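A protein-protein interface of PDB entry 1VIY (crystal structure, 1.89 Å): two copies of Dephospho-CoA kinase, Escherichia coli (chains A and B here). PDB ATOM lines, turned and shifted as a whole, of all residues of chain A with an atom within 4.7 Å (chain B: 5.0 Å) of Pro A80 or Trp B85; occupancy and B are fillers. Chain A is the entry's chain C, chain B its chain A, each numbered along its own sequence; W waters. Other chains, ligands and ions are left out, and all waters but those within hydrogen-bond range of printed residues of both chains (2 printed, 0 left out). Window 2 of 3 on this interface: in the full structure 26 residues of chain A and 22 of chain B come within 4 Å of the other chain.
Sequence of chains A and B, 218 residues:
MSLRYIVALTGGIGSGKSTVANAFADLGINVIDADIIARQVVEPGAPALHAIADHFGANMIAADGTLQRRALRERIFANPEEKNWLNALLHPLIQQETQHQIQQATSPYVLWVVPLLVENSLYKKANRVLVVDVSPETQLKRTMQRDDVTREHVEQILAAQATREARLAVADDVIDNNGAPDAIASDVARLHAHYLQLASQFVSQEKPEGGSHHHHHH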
ATOM      1  N   ALA A  78      17.741 -15.588  -9.210  1.00  0.00           N
ATOM      2  CA  ALA A  78      17.665 -15.520  -7.741  1.00  0.00           C
ATOM      3  C   ALA A  78      16.419 -14.721  -7.330  1.00  0.00           C
ATOM      4  O   ALA A  78      16.406 -14.007  -6.293  1.00  0.00           O
ATOM      5  CB  ALA A  78      18.915 -14.884  -7.164  1.00  0.00           C
ATOM      6  N   ASN A  79      15.382 -14.833  -8.151  1.00  0.00           N
ATOM      7  CA  ASN A  79      14.137 -14.137  -7.853  1.00  0.00           C
ATOM      8  C   ASN A  79      12.904 -15.002  -8.129  1.00  0.00           C
ATOM      9  O   ASN A  79      12.295 -14.905  -9.210  1.00  0.00           O
ATOM     10  CB  ASN A  79      14.080 -12.840  -8.666  1.00  0.00           C
ATOM     11  CG  ASN A  79      13.052 -11.866  -8.142  1.00  0.00           C
ATOM     12  OD1 ASN A  79      11.901 -12.227  -7.856  1.00  0.00           O
ATOM     13  ND2 ASN A  79      13.468 -10.624  -8.005  1.00  0.00           N
ATOM     14  N   PRO A  80      12.498 -15.798  -7.143  1.00  0.00           N
ATOM     15  CA  PRO A  80      11.386 -16.741  -7.320  1.00  0.00           C
ATOM     16  C   PRO A  80      10.054 -16.050  -7.696  1.00  0.00           C
ATOM     17  O   PRO A  80       9.268 -16.627  -8.474  1.00  0.00           O
ATOM     18  CB  PRO A  80      11.273 -17.390  -5.937  1.00  0.00           C
ATOM     19  CG  PRO A  80      12.692 -17.269  -5.369  1.00  0.00           C
ATOM     20  CD  PRO A  80      13.079 -15.890  -5.787  1.00  0.00           C
ATOM     21  N   GLU A  81       9.809 -14.855  -7.158  1.00  0.00           N
ATOM     22  CA  GLU A  81       8.569 -14.115  -7.452  1.00  0.00           C
ATOM     23  C   GLU A  81       8.489 -13.721  -8.935  1.00  0.00           C
ATOM     24  O   GLU A  81       7.432 -13.857  -9.561  1.00  0.00           O
ATOM     25  CB  GLU A  81       8.412 -12.893  -6.535  1.00  0.00           C
ATOM     26  CG  GLU A  81       8.018 -13.230  -5.107  1.00  0.00           C
ATOM     27  CD  GLU A  81       8.180 -12.058  -4.114  1.00  0.00           C
ATOM     28  OE1 GLU A  81       8.719 -10.990  -4.475  1.00  0.00           O
ATOM     29  OE2 GLU A  81       7.782 -12.223  -2.945  1.00  0.00           O
ATOM     30  N   GLU A  82       9.612 -13.280  -9.496  1.00  0.00           N
ATOM     31  CA  GLU A  82       9.671 -12.864 -10.905  1.00  0.00           C
ATOM     32  C   GLU A  82       9.647 -14.097 -11.841  1.00  0.00           C
ATOM     33  O   GLU A  82       9.041 -14.067 -12.909  1.00  0.00           O
ATOM     34  CB  GLU A  82      10.932 -12.022 -11.162  1.00  0.00           C
ATOM     35  CG  GLU A  82      10.872 -10.569 -10.679  1.00  0.00           C
ATOM     36  CD  GLU A  82       9.861  -9.727 -11.449  1.00  0.00           C
ATOM     37  OE1 GLU A  82       8.663 -10.097 -11.510  1.00  0.00           O
ATOM     38  OE2 GLU A  82      10.279  -8.696 -12.034  1.00  0.00           O
ATOM     39  N   LYS A  83      10.296 -15.175 -11.404  1.00  0.00           N
ATOM     40  CA  LYS A  83      10.261 -16.449 -12.107  1.00  0.00           C
ATOM     41  C   LYS A  83       8.837 -16.992 -12.099  1.00  0.00           C
ATOM     42  O   LYS A  83       8.327 -17.410 -13.142  1.00  0.00           O
ATOM     43  CB  LYS A  83      11.212 -17.451 -11.449  1.00  0.00           C
ATOM     44  CG  LYS A  83      11.070 -18.898 -11.930  1.00  0.00           C
ATOM     45  CD  LYS A  83      12.273 -19.720 -11.411  1.00  0.00           C
ATOM     46  CE  LYS A  83      12.240 -21.194 -11.809  1.00  0.00           C
ATOM     47  NZ  LYS A  83      13.492 -21.888 -11.307  1.00  0.00           N
ATOM     48  N   ASN A  84       8.197 -16.949 -10.934  1.00  0.00           N
ATOM     49  CA  ASN A  84       6.791 -17.329 -10.816  1.00  0.00           C
ATOM     50  C   ASN A  84       5.860 -16.518 -11.712  1.00  0.00           C
ATOM     51  O   ASN A  84       4.936 -17.075 -12.304  1.00  0.00           O
ATOM     52  CB  ASN A  84       6.337 -17.265  -9.358  1.00  0.00           C
ATOM     53  CG  ASN A  84       6.857 -18.461  -8.542  1.00  0.00           C
ATOM     54  OD1 ASN A  84       7.376 -19.413  -9.109  1.00  0.00           O
ATOM     55  ND2 ASN A  84       6.716 -18.407  -7.225  1.00  0.00           N
ATOM     56  N   ALA B  51      19.625 -12.301  -1.766  1.00  0.00           N
ATOM     57  CA  ALA B  51      18.180 -12.391  -2.022  1.00  0.00           C
ATOM     58  C   ALA B  51      17.399 -12.602  -0.738  1.00  0.00           C
ATOM     59  O   ALA B  51      16.315 -12.071  -0.604  1.00  0.00           O
ATOM     60  CB  ALA B  51      17.867 -13.483  -3.023  1.00  0.00           C
ATOM     61  N   ILE B  52      17.962 -13.356   0.212  1.00  0.00           N
ATOM     62  CA  ILE B  52      17.287 -13.533   1.516  1.00  0.00           C
ATOM     63  C   ILE B  52      17.181 -12.195   2.250  1.00  0.00           C
ATOM     64  O   ILE B  52      16.118 -11.840   2.821  1.00  0.00           O
ATOM     65  CB  ILE B  52      18.011 -14.591   2.381  1.00  0.00           C
ATOM     66  CG1 ILE B  52      17.736 -15.983   1.813  1.00  0.00           C
ATOM     67  CG2 ILE B  52      17.550 -14.454   3.888  1.00  0.00           C
ATOM     68  CD1 ILE B  52      18.746 -17.048   2.303  1.00  0.00           C
ATOM     69  N   HIS B  55      14.598  -9.982   0.594  1.00  0.00           N
ATOM     70  CA  HIS B  55      13.229 -10.493   0.778  1.00  0.00           C
ATOM     71  C   HIS B  55      12.727 -10.303   2.193  1.00  0.00           C
ATOM     72  O   HIS B  55      11.580  -9.878   2.403  1.00  0.00           O
ATOM     73  CB  HIS B  55      13.163 -11.974   0.411  1.00  0.00           C
ATOM     74  CG  HIS B  55      11.778 -12.537   0.378  1.00  0.00           C
ATOM     75  ND1 HIS B  55      10.901 -12.293  -0.655  1.00  0.00           N
ATOM     76  CD2 HIS B  55      11.131 -13.369   1.232  1.00  0.00           C
ATOM     77  CE1 HIS B  55       9.761 -12.924  -0.426  1.00  0.00           C
ATOM     78  NE2 HIS B  55       9.867 -13.576   0.720  1.00  0.00           N
ATOM     79  N   PHE B  56      13.577 -10.605   3.162  1.00  0.00           N
ATOM     80  CA  PHE B  56      13.138 -10.623   4.569  1.00  0.00           C
ATOM     81  C   PHE B  56      13.617  -9.376   5.327  1.00  0.00           C
ATOM     82  O   PHE B  56      13.063  -9.016   6.360  1.00  0.00           O
ATOM     83  CB  PHE B  56      13.631 -11.884   5.280  1.00  0.00           C
ATOM     84  CG  PHE B  56      13.024 -13.196   4.765  1.00  0.00           C
ATOM     85  CD1 PHE B  56      11.788 -13.638   5.232  1.00  0.00           C
ATOM     86  CD2 PHE B  56      13.719 -14.003   3.873  1.00  0.00           C
ATOM     87  CE1 PHE B  56      11.249 -14.865   4.785  1.00  0.00           C
ATOM     88  CE2 PHE B  56      13.202 -15.217   3.406  1.00  0.00           C
ATOM     89  CZ  PHE B  56      11.956 -15.662   3.874  1.00  0.00           C
ATOM     90  N   GLU B  81       4.443 -20.207   4.446  1.00  0.00           N
ATOM     91  CA  GLU B  81       4.545 -20.137   2.981  1.00  0.00           C
ATOM     92  C   GLU B  81       5.850 -19.483   2.497  1.00  0.00           C
ATOM     93  O   GLU B  81       6.158 -19.481   1.295  1.00  0.00           O
ATOM     94  CB  GLU B  81       3.343 -19.333   2.436  1.00  0.00           C
ATOM     95  CG  GLU B  81       3.292 -17.883   2.930  1.00  0.00           C
ATOM     96  CD  GLU B  81       2.026 -17.126   2.542  1.00  0.00           C
ATOM     97  OE1 GLU B  81       1.777 -16.904   1.331  1.00  0.00           O
ATOM     98  OE2 GLU B  81       1.284 -16.724   3.465  1.00  0.00           O
ATOM     99  N   GLU B  82       6.616 -18.906   3.425  1.00  0.00           N
ATOM    100  CA  GLU B  82       7.918 -18.366   3.086  1.00  0.00           C
ATOM    101  C   GLU B  82       8.901 -19.530   2.858  1.00  0.00           C
ATOM    102  O   GLU B  82       9.884 -19.396   2.118  1.00  0.00           O
ATOM    103  CB  GLU B  82       8.418 -17.416   4.182  1.00  0.00           C
ATOM    104  CG  GLU B  82       7.638 -16.120   4.323  1.00  0.00           C
ATOM    105  CD  GLU B  82       7.929 -15.108   3.213  1.00  0.00           C
ATOM    106  OE1 GLU B  82       8.181 -15.504   2.044  1.00  0.00           O
ATOM    107  OE2 GLU B  82       7.894 -13.899   3.513  1.00  0.00           O
ATOM    108  N   LYS B  83       8.618 -20.673   3.479  1.00  0.00           N
ATOM    109  CA  LYS B  83       9.406 -21.885   3.254  1.00  0.00           C
ATOM    110  C   LYS B  83       9.471 -22.212   1.772  1.00  0.00           C
ATOM    111  O   LYS B  83      10.526 -22.543   1.241  1.00  0.00           O
ATOM    112  CB  LYS B  83       8.765 -23.053   3.985  1.00  0.00           C
ATOM    113  CG  LYS B  83       9.600 -23.649   5.047  1.00  0.00           C
ATOM    114  CD  LYS B  83       9.006 -24.997   5.530  1.00  0.00           C
ATOM    115  CE  LYS B  83       7.512 -24.895   5.941  1.00  0.00           C
ATOM    116  NZ  LYS B  83       7.346 -24.273   7.284  1.00  0.00           N
ATOM    117  N   ASN B  84       8.323 -22.099   1.115  1.00  0.00           N
ATOM    118  CA  ASN B  84       8.213 -22.323  -0.312  1.00  0.00           C
ATOM    119  C   ASN B  84       9.047 -21.308  -1.105  1.00  0.00           C
ATOM    120  O   ASN B  84       9.756 -21.694  -2.069  1.00  0.00           O
ATOM    121  CB  ASN B  84       6.752 -22.314  -0.737  1.00  0.00           C
ATOM    122  CG  ASN B  84       5.933 -23.417  -0.051  1.00  0.00           C
ATOM    123  OD1 ASN B  84       6.421 -24.521   0.175  1.00  0.00           O
ATOM    124  ND2 ASN B  84       4.702 -23.095   0.324  1.00  0.00           N
ATOM    125  N   TRP B  85       9.014 -20.035  -0.676  1.00  0.00           N
ATOM    126  CA  TRP B  85       9.824 -18.991  -1.350  1.00  0.00           C
ATOM    127  C   TRP B  85      11.294 -19.378  -1.215  1.00  0.00           C
ATOM    128  O   TRP B  85      12.034 -19.376  -2.197  1.00  0.00           O
ATOM    129  CB  TRP B  85       9.567 -17.580  -0.760  1.00  0.00           C
ATOM    130  CG  TRP B  85      10.393 -16.507  -1.445  1.00  0.00           C
ATOM    131  CD1 TRP B  85      10.035 -15.759  -2.528  1.00  0.00           C
ATOM    132  CD2 TRP B  85      11.732 -16.101  -1.109  1.00  0.00           C
ATOM    133  NE1 TRP B  85      11.061 -14.903  -2.876  1.00  0.00           N
ATOM    134  CE2 TRP B  85      12.104 -15.082  -2.007  1.00  0.00           C
ATOM    135  CE3 TRP B  85      12.630 -16.445  -0.093  1.00  0.00           C
ATOM    136  CZ2 TRP B  85      13.355 -14.467  -1.967  1.00  0.00           C
ATOM    137  CZ3 TRP B  85      13.883 -15.840  -0.076  1.00  0.00           C
ATOM    138  CH2 TRP B  85      14.211 -14.849  -0.985  1.00  0.00           C
ATOM    139  N   LEU B  86      11.694 -19.732  -0.003  1.00  0.00           N
ATOM    140  CA  LEU B  86      13.084 -20.101   0.316  1.00  0.00           C
ATOM    141  C   LEU B  86      13.583 -21.322  -0.462  1.00  0.00           C
ATOM    142  O   LEU B  86      14.662 -21.277  -1.075  1.00  0.00           O
ATOM    143  CB  LEU B  86      13.276 -20.261   1.849  1.00  0.00           C
ATOM    144  CG  LEU B  86      14.693 -20.438   2.389  1.00  0.00           C
ATOM    145  CD1 LEU B  86      15.580 -19.159   2.147  1.00  0.00           C
ATOM    146  CD2 LEU B  86      14.697 -20.831   3.884  1.00  0.00           C
ATOM    147  N   ASN B  87      12.798 -22.403  -0.460  1.00  0.00           N
ATOM    148  CA  ASN B  87      13.123 -23.553  -1.293  1.00  0.00           C
ATOM    149  C   ASN B  87      13.257 -23.226  -2.775  1.00  0.00           C
ATOM    150  O   ASN B  87      14.180 -23.752  -3.432  1.00  0.00           O
ATOM    151  CB  ASN B  87      12.146 -24.747  -1.061  1.00  0.00           C
ATOM    152  CG  ASN B  87      12.360 -25.421   0.302  1.00  0.00           C
ATOM    153  OD1 ASN B  87      13.464 -25.374   0.876  1.00  0.00           O
ATOM    154  ND2 ASN B  87      11.314 -26.032   0.827  1.00  0.00           N
ATOM    155  N   ALA B  88      12.339 -22.405  -3.309  1.00  0.00           N
ATOM    156  CA  ALA B  88      12.363 -21.993  -4.723  1.00  0.00           C
ATOM    157  C   ALA B  88      13.626 -21.185  -5.060  1.00  0.00           C
ATOM    158  O   ALA B  88      14.194 -21.308  -6.128  1.00  0.00           O
ATOM    159  CB  ALA B  88      11.107 -21.163  -5.053  1.00  0.00           C
ATOM    160  N   LEU B  89      14.061 -20.352  -4.123  1.00  0.00           N
ATOM    161  CA  LEU B  89      15.277 -19.574  -4.309  1.00  0.00           C
ATOM    162  C   LEU B  89      16.488 -20.534  -4.362  1.00  0.00           C
ATOM    163  O   LEU B  89      17.284 -20.496  -5.289  1.00  0.00           O
ATOM    164  CB  LEU B  89      15.451 -18.577  -3.147  1.00  0.00           C
ATOM    165  CG  LEU B  89      16.838 -17.876  -3.087  1.00  0.00           C
ATOM    166  CD1 LEU B  89      16.975 -16.897  -4.245  1.00  0.00           C
ATOM    167  CD2 LEU B  89      17.060 -17.171  -1.713  1.00  0.00           C
HETATM  168  O   HOH W   1      13.397 -21.539  -8.429  1.00  0.00           O
HETATM  169  O   HOH W   2      11.430 -13.003  -5.069  1.00  0.00           O
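Of chain B, only Trp B85, Ala B88 and Leu B89 come within 4 Å of Pro A80. Of chain A, only Pro A80 (3.7 Å) comes within 4 Å of Trp B85. Printed residues of chain A within 4 Å of Ala B51: Ala A78 (3.6 Å). Printed residues of chain B within 4 Å of Glu A81: His B55 (3.3 Å). Glu B82 touches none of the printed residues of chain A. The nearest residue of chain A that does not touch Trp B85 is Glu A81 (4.1 Å). The nearest printed residue of chain A that does not touch Ala B51 is Asn A79 (5.9 Å).
Ala A78 touches Ala B51 (O to CB, 3.6 Å). Ala A78 touches Leu B89. Trp B85 touches Pro A80. Pro A80 touches Ala B88. N of Leu B89 touches CG of Pro A80 (3.6 Å). His B55 touches Glu A81 (CE1 to OE2, 3.3 Å).
The side-chain carboxylate (OE1) of Glu B82 is in hydrogen-bond range of a ring nitrogen (NE2) of His B55, 2.9 Å away. The indole nitrogen (NE1) of Trp B85 lies close to a ring nitrogen (ND1) of His B55. The backbone NH (N) of Glu A81 lies close to the side-chain amide oxygen (OD1) of Asn A79, at 3.4 Å. ND2 of Asn A84 lies close to O of Pro A80 (3.4 Å).
Water W1 lies within hydrogen-bond range of O of Ala B88 and NZ of Lys A83. Water W2 lies within hydrogen-bond range of NE1 of Trp B85 (2.9 Å), OD1 of Asn A79 (2.9 Å) and N of Glu A81 (3.2 Å).
Hydrophobic or aromatic side chains of chain A within 4 Å of the printed part of chain B: Pro A80. Hydrophobic or aromatic side chains of chain B that line the printed part of chain A: Ala B51, His B55, Trp B85, Ala B88 and Leu B89. Among the printed residues, 6 pairs touch across the chains.
Positions printed for both chains: 81, 82, 83 and 84.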
